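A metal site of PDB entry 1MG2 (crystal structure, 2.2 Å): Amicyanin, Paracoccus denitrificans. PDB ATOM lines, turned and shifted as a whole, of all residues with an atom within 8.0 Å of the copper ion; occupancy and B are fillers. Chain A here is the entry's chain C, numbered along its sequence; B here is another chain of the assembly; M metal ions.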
ATOM      1  N   ILE A  25      17.029  15.754 -19.786  1.00  0.00           N
ATOM      2  CA  ILE A  25      16.991  14.325 -20.062  1.00  0.00           C
ATOM      3  C   ILE A  25      15.603  13.821 -19.707  1.00  0.00           C
ATOM      4  O   ILE A  25      15.155  13.950 -18.575  1.00  0.00           O
ATOM      5  CB  ILE A  25      18.020  13.546 -19.222  1.00  0.00           C
ATOM      6  CG1 ILE A  25      19.405  14.199 -19.347  1.00  0.00           C
ATOM      7  CG2 ILE A  25      18.077  12.103 -19.684  1.00  0.00           C
ATOM      8  CD1 ILE A  25      20.489  13.500 -18.538  1.00  0.00           C
ATOM      9  N   MET A  28      13.792   8.655 -22.096  1.00  0.00           N
ATOM     10  CA  MET A  28      14.906   7.863 -22.572  1.00  0.00           C
ATOM     11  C   MET A  28      15.818   8.564 -23.570  1.00  0.00           C
ATOM     12  O   MET A  28      16.381   7.925 -24.448  1.00  0.00           O
ATOM     13  CB  MET A  28      14.383   6.578 -23.228  1.00  0.00           C
ATOM     14  CG  MET A  28      13.482   5.735 -22.347  1.00  0.00           C
ATOM     15  SD  MET A  28      14.311   5.229 -20.835  1.00  0.00           S
ATOM     16  CE  MET A  28      15.314   3.909 -21.462  1.00  0.00           C
ATOM     17  N   LYS A  29      15.971   9.884 -23.444  1.00  0.00           N
ATOM     18  CA  LYS A  29      16.858  10.585 -24.374  1.00  0.00           C
ATOM     19  C   LYS A  29      17.285  11.976 -23.942  1.00  0.00           C
ATOM     20  O   LYS A  29      16.624  12.628 -23.139  1.00  0.00           O
ATOM     21  CB  LYS A  29      16.226  10.655 -25.767  1.00  0.00           C
ATOM     22  CG  LYS A  29      14.915  11.431 -25.847  1.00  0.00           C
ATOM     23  CD  LYS A  29      14.244  11.237 -27.205  1.00  0.00           C
ATOM     24  CE  LYS A  29      12.841  11.812 -27.232  1.00  0.00           C
ATOM     25  NZ  LYS A  29      12.841  13.272 -26.919  1.00  0.00           N
ATOM     26  N   TYR A  30      18.421  12.404 -24.500  1.00  0.00           N
ATOM     27  CA  TYR A  30      18.967  13.729 -24.243  1.00  0.00           C
ATOM     28  C   TYR A  30      18.196  14.619 -25.215  1.00  0.00           C
ATOM     29  O   TYR A  30      18.454  14.606 -26.422  1.00  0.00           O
ATOM     30  CB  TYR A  30      20.463  13.752 -24.584  1.00  0.00           C
ATOM     31  CG  TYR A  30      21.287  12.758 -23.776  1.00  0.00           C
ATOM     32  CD1 TYR A  30      21.414  12.897 -22.396  1.00  0.00           C
ATOM     33  CD2 TYR A  30      21.934  11.679 -24.401  1.00  0.00           C
ATOM     34  CE1 TYR A  30      22.170  11.995 -21.647  1.00  0.00           C
ATOM     35  CE2 TYR A  30      22.697  10.771 -23.657  1.00  0.00           C
ATOM     36  CZ  TYR A  30      22.805  10.937 -22.273  1.00  0.00           C
ATOM     37  OH  TYR A  30      23.557  10.075 -21.512  1.00  0.00           O
ATOM     38  N   ASN A  47      18.164  15.657 -15.224  1.00  0.00           N
ATOM     39  CA  ASN A  47      17.246  14.549 -15.454  1.00  0.00           C
ATOM     40  C   ASN A  47      15.851  14.995 -15.017  1.00  0.00           C
ATOM     41  O   ASN A  47      15.652  15.474 -13.899  1.00  0.00           O
ATOM     42  CB  ASN A  47      17.691  13.317 -14.679  1.00  0.00           C
ATOM     43  CG  ASN A  47      16.848  12.085 -14.998  1.00  0.00           C
ATOM     44  OD1 ASN A  47      16.074  12.093 -15.951  1.00  0.00           O
ATOM     45  ND2 ASN A  47      17.005  11.035 -14.200  1.00  0.00           N
ATOM     46  N   GLU A  49      13.040  12.855 -15.376  1.00  0.00           N
ATOM     47  CA  GLU A  49      12.166  11.714 -15.158  1.00  0.00           C
ATOM     48  C   GLU A  49      12.646  10.787 -14.044  1.00  0.00           C
ATOM     49  O   GLU A  49      13.759  10.949 -13.531  1.00  0.00           O
ATOM     50  CB  GLU A  49      11.987  10.929 -16.463  1.00  0.00           C
ATOM     51  CG  GLU A  49      13.231  10.204 -16.951  1.00  0.00           C
ATOM     52  CD  GLU A  49      13.022   9.524 -18.295  1.00  0.00           C
ATOM     53  OE1 GLU A  49      11.895   9.041 -18.560  1.00  0.00           O
ATOM     54  OE2 GLU A  49      13.975   9.465 -19.097  1.00  0.00           O
ATOM     55  N   MET A  51      13.381   7.559 -14.258  1.00  0.00           N
ATOM     56  CA  MET A  51      14.450   6.697 -14.763  1.00  0.00           C
ATOM     57  C   MET A  51      15.799   7.395 -14.588  1.00  0.00           C
ATOM     58  O   MET A  51      16.025   8.472 -15.121  1.00  0.00           O
ATOM     59  CB  MET A  51      14.215   6.402 -16.252  1.00  0.00           C
ATOM     60  CG  MET A  51      15.279   5.549 -16.946  1.00  0.00           C
ATOM     61  SD  MET A  51      15.078   3.791 -16.632  1.00  0.00           S
ATOM     62  CE  MET A  51      13.733   3.412 -17.754  1.00  0.00           C
ATOM     63  N   PRO A  52      16.719   6.783 -13.826  1.00  0.00           N
ATOM     64  CA  PRO A  52      18.037   7.406 -13.631  1.00  0.00           C
ATOM     65  C   PRO A  52      18.863   7.436 -14.919  1.00  0.00           C
ATOM     66  O   PRO A  52      18.763   6.534 -15.755  1.00  0.00           O
ATOM     67  CB  PRO A  52      18.674   6.525 -12.547  1.00  0.00           C
ATOM     68  CG  PRO A  52      17.481   6.038 -11.771  1.00  0.00           C
ATOM     69  CD  PRO A  52      16.507   5.679 -12.874  1.00  0.00           C
ATOM     70  N   HIS A  53      19.681   8.465 -15.068  1.00  0.00           N
ATOM     71  CA  HIS A  53      20.520   8.618 -16.264  1.00  0.00           C
ATOM     72  C   HIS A  53      21.812   9.319 -15.857  1.00  0.00           C
ATOM     73  O   HIS A  53      21.906   9.894 -14.777  1.00  0.00           O
ATOM     74  CB  HIS A  53      19.817   9.490 -17.307  1.00  0.00           C
ATOM     75  CG  HIS A  53      18.505   8.956 -17.790  1.00  0.00           C
ATOM     76  ND1 HIS A  53      18.372   7.878 -18.641  1.00  0.00           N
ATOM     77  CD2 HIS A  53      17.242   9.395 -17.576  1.00  0.00           C
ATOM     78  CE1 HIS A  53      17.072   7.714 -18.916  1.00  0.00           C
ATOM     79  NE2 HIS A  53      16.347   8.615 -18.285  1.00  0.00           N
ATOM     80  N   ASN A  54      22.812   9.268 -16.725  1.00  0.00           N
ATOM     81  CA  ASN A  54      24.086   9.942 -16.463  1.00  0.00           C
ATOM     82  C   ASN A  54      24.696  10.303 -17.818  1.00  0.00           C
ATOM     83  O   ASN A  54      24.049  10.175 -18.853  1.00  0.00           O
ATOM     84  CB  ASN A  54      25.028   9.007 -15.698  1.00  0.00           C
ATOM     85  CG  ASN A  54      25.697   7.984 -16.593  1.00  0.00           C
ATOM     86  OD1 ASN A  54      25.062   7.430 -17.497  1.00  0.00           O
ATOM     87  ND2 ASN A  54      26.978   7.714 -16.355  1.00  0.00           N
ATOM     88  N   VAL A  55      25.939  10.790 -17.790  1.00  0.00           N
ATOM     89  CA  VAL A  55      26.643  11.122 -19.014  1.00  0.00           C
ATOM     90  C   VAL A  55      27.926  10.306 -18.930  1.00  0.00           C
ATOM     91  O   VAL A  55      28.561  10.247 -17.887  1.00  0.00           O
ATOM     92  CB  VAL A  55      26.975  12.633 -19.144  1.00  0.00           C
ATOM     93  CG1 VAL A  55      25.696  13.427 -19.304  1.00  0.00           C
ATOM     94  CG2 VAL A  55      27.754  13.116 -17.940  1.00  0.00           C
ATOM     95  N   MET A  71      24.976   8.847 -11.681  1.00  0.00           N
ATOM     96  CA  MET A  71      23.593   8.750 -12.116  1.00  0.00           C
ATOM     97  C   MET A  71      22.809   9.910 -11.531  1.00  0.00           C
ATOM     98  O   MET A  71      23.000  10.277 -10.366  1.00  0.00           O
ATOM     99  CB  MET A  71      22.972   7.430 -11.654  1.00  0.00           C
ATOM    100  CG  MET A  71      23.570   6.199 -12.304  1.00  0.00           C
ATOM    101  SD  MET A  71      23.441   6.227 -14.097  1.00  0.00           S
ATOM    102  CE  MET A  71      21.698   6.064 -14.307  1.00  0.00           C
ATOM    103  N   MET A  72      21.917  10.484 -12.338  1.00  0.00           N
ATOM    104  CA  MET A  72      21.091  11.597 -11.891  1.00  0.00           C
ATOM    105  C   MET A  72      19.675  11.098 -11.691  1.00  0.00           C
ATOM    106  O   MET A  72      19.093  10.495 -12.587  1.00  0.00           O
ATOM    107  CB  MET A  72      21.075  12.718 -12.944  1.00  0.00           C
ATOM    108  CG  MET A  72      22.400  13.428 -13.164  1.00  0.00           C
ATOM    109  SD  MET A  72      22.357  14.593 -14.568  1.00  0.00           S
ATOM    110  CE  MET A  72      23.056  13.543 -15.859  1.00  0.00           C
ATOM    111  N   HIS A  91      27.295   9.006 -23.896  1.00  0.00           N
ATOM    112  CA  HIS A  91      26.113   8.156 -23.813  1.00  0.00           C
ATOM    113  C   HIS A  91      25.782   7.865 -22.361  1.00  0.00           C
ATOM    114  O   HIS A  91      26.527   8.243 -21.449  1.00  0.00           O
ATOM    115  CB  HIS A  91      26.366   6.829 -24.546  1.00  0.00           C
ATOM    116  CG  HIS A  91      27.332   5.921 -23.843  1.00  0.00           C
ATOM    117  ND1 HIS A  91      28.699   6.129 -23.862  1.00  0.00           N
ATOM    118  CD2 HIS A  91      27.131   4.810 -23.102  1.00  0.00           C
ATOM    119  CE1 HIS A  91      29.296   5.174 -23.162  1.00  0.00           C
ATOM    120  NE2 HIS A  91      28.361   4.361 -22.689  1.00  0.00           N
ATOM    121  N   CYS A  92      24.650   7.202 -22.144  1.00  0.00           N
ATOM    122  CA  CYS A  92      24.225   6.831 -20.801  1.00  0.00           C
ATOM    123  C   CYS A  92      24.717   5.401 -20.539  1.00  0.00           C
ATOM    124  O   CYS A  92      24.385   4.478 -21.268  1.00  0.00           O
ATOM    125  CB  CYS A  92      22.694   6.893 -20.719  1.00  0.00           C
ATOM    126  SG  CYS A  92      22.067   6.774 -19.049  1.00  0.00           S
ATOM    127  N   THR A  93      25.513   5.228 -19.488  1.00  0.00           N
ATOM    128  CA  THR A  93      26.081   3.909 -19.178  1.00  0.00           C
ATOM    129  C   THR A  93      25.116   2.708 -19.329  1.00  0.00           C
ATOM    130  O   THR A  93      25.331   1.849 -20.193  1.00  0.00           O
ATOM    131  CB  THR A  93      26.705   3.897 -17.756  1.00  0.00           C
ATOM    132  OG1 THR A  93      27.896   4.688 -17.756  1.00  0.00           O
ATOM    133  CG2 THR A  93      27.054   2.474 -17.332  1.00  0.00           C
ATOM    134  N   PRO A  94      24.048   2.651 -18.522  1.00  0.00           N
ATOM    135  CA  PRO A  94      23.098   1.531 -18.615  1.00  0.00           C
ATOM    136  C   PRO A  94      22.235   1.547 -19.863  1.00  0.00           C
ATOM    137  O   PRO A  94      21.563   0.564 -20.171  1.00  0.00           O
ATOM    138  CB  PRO A  94      22.269   1.699 -17.347  1.00  0.00           C
ATOM    139  CG  PRO A  94      22.129   3.171 -17.281  1.00  0.00           C
ATOM    140  CD  PRO A  94      23.551   3.658 -17.566  1.00  0.00           C
ATOM    141  N   HIS A  95      22.233   2.682 -20.569  1.00  0.00           N
ATOM    142  CA  HIS A  95      21.421   2.838 -21.775  1.00  0.00           C
ATOM    143  C   HIS A  95      22.301   3.286 -22.933  1.00  0.00           C
ATOM    144  O   HIS A  95      22.252   4.449 -23.336  1.00  0.00           O
ATOM    145  CB  HIS A  95      20.333   3.884 -21.513  1.00  0.00           C
ATOM    146  CG  HIS A  95      19.554   3.658 -20.249  1.00  0.00           C
ATOM    147  ND1 HIS A  95      18.804   4.625 -19.624  1.00  0.00           N
ATOM    148  CD2 HIS A  95      19.420   2.540 -19.486  1.00  0.00           C
ATOM    149  CE1 HIS A  95      18.256   4.083 -18.524  1.00  0.00           C
ATOM    150  NE2 HIS A  95      18.599   2.818 -18.400  1.00  0.00           N
ATOM    151  N   PRO A  96      23.117   2.378 -23.485  1.00  0.00           N
ATOM    152  CA  PRO A  96      24.017   2.682 -24.595  1.00  0.00           C
ATOM    153  C   PRO A  96      23.343   3.317 -25.811  1.00  0.00           C
ATOM    154  O   PRO A  96      24.000   3.947 -26.636  1.00  0.00           O
ATOM    155  CB  PRO A  96      24.646   1.327 -24.926  1.00  0.00           C
ATOM    156  CG  PRO A  96      24.663   0.629 -23.590  1.00  0.00           C
ATOM    157  CD  PRO A  96      23.279   0.964 -23.071  1.00  0.00           C
ATOM    158  N   PHE A  97      22.029   3.143 -25.923  1.00  0.00           N
ATOM    159  CA  PHE A  97      21.298   3.718 -27.046  1.00  0.00           C
ATOM    160  C   PHE A  97      21.078   5.222 -26.877  1.00  0.00           C
ATOM    161  O   PHE A  97      20.857   5.928 -27.863  1.00  0.00           O
ATOM    162  CB  PHE A  97      19.953   3.004 -27.238  1.00  0.00           C
ATOM    163  CG  PHE A  97      19.179   2.824 -25.977  1.00  0.00           C
ATOM    164  CD1 PHE A  97      19.589   1.906 -25.020  1.00  0.00           C
ATOM    165  CD2 PHE A  97      18.032   3.564 -25.748  1.00  0.00           C
ATOM    166  CE1 PHE A  97      18.855   1.725 -23.847  1.00  0.00           C
ATOM    167  CE2 PHE A  97      17.292   3.399 -24.580  1.00  0.00           C
ATOM    168  CZ  PHE A  97      17.709   2.475 -23.627  1.00  0.00           C
ATOM    169  N   MET A  98      21.122   5.713 -25.646  1.00  0.00           N
ATOM    170  CA  MET A  98      20.972   7.149 -25.402  1.00  0.00           C
ATOM    171  C   MET A  98      22.298   7.806 -25.771  1.00  0.00           C
ATOM    172  O   MET A  98      23.284   7.687 -25.037  1.00  0.00           O
ATOM    173  CB  MET A  98      20.647   7.422 -23.932  1.00  0.00           C
ATOM    174  CG  MET A  98      19.212   7.128 -23.549  1.00  0.00           C
ATOM    175  SD  MET A  98      18.907   7.404 -21.793  1.00  0.00           S
ATOM    176  CE  MET A  98      18.933   9.178 -21.724  1.00  0.00           C
ATOM    177  N   SER B  56      21.657   0.591 -13.127  1.00  0.00           N
ATOM    178  CA  SER B  56      20.813  -0.550 -12.821  1.00  0.00           C
ATOM    179  C   SER B  56      19.628  -0.657 -13.763  1.00  0.00           C
ATOM    180  O   SER B  56      19.420   0.202 -14.628  1.00  0.00           O
ATOM    181  CB  SER B  56      20.262  -0.454 -11.398  1.00  0.00           C
ATOM    182  OG  SER B  56      19.200   0.490 -11.343  1.00  0.00           O
ATOM    183  N   GLU B 101      17.021  -1.158 -20.176  1.00  0.00           N
ATOM    184  CA  GLU B 101      16.534  -0.351 -19.057  1.00  0.00           C
ATOM    185  C   GLU B 101      15.579  -1.117 -18.155  1.00  0.00           C
ATOM    186  O   GLU B 101      15.422  -0.774 -16.987  1.00  0.00           O
ATOM    187  CB  GLU B 101      15.848   0.933 -19.567  1.00  0.00           C
ATOM    188  CG  GLU B 101      14.596   0.689 -20.407  1.00  0.00           C
ATOM    189  CD  GLU B 101      14.895   0.543 -21.892  1.00  0.00           C
ATOM    190  OE1 GLU B 101      15.999   0.078 -22.250  1.00  0.00           O
ATOM    191  OE2 GLU B 101      14.011   0.890 -22.700  1.00  0.00           O
HETATM  192 CU    CU M   1      19.892   6.516 -19.345  1.00  0.00          CU
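A ring nitrogen (NE2) of His 53 sits close to the backbone carbonyl oxygen of Met 51, at 3.2 Å.
The side-chain sulfur (SG) of Cys 92 sits close to the side-chain amide oxygen (OD1) of Asn 54 (3.4 Å).
NE2 of His 53 lies within hydrogen-bond range of OE2 of Glu 49 (2.6 Å).
The side-chain hydroxyl of Tyr 30 sits at hydrogen-bond distance from the backbone NH of Cys 92, 3.1 Å away.
O of His 53 lies within hydrogen-bond range of N of Met 72 (2.5 Å).
Pro 52 touches the copper ion.
Of the 23 residues printed, 5 come within 4 Å of the copper ion.
The nearest printed residue that does not touch the copper ion is Pro 94 (4.5 Å).
The copper ion is bound by a ring nitrogen (ND1) of His 53 (2.2 Å), a ring nitrogen (ND1) of His 95 (2.2 Å), the side-chain sulfur (SG) of Cys 92 (2.2 Å) and the side-chain sulfur (SD) of Met 98 (2.8 Å).
The copper ion has four donor atoms within binding distance.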
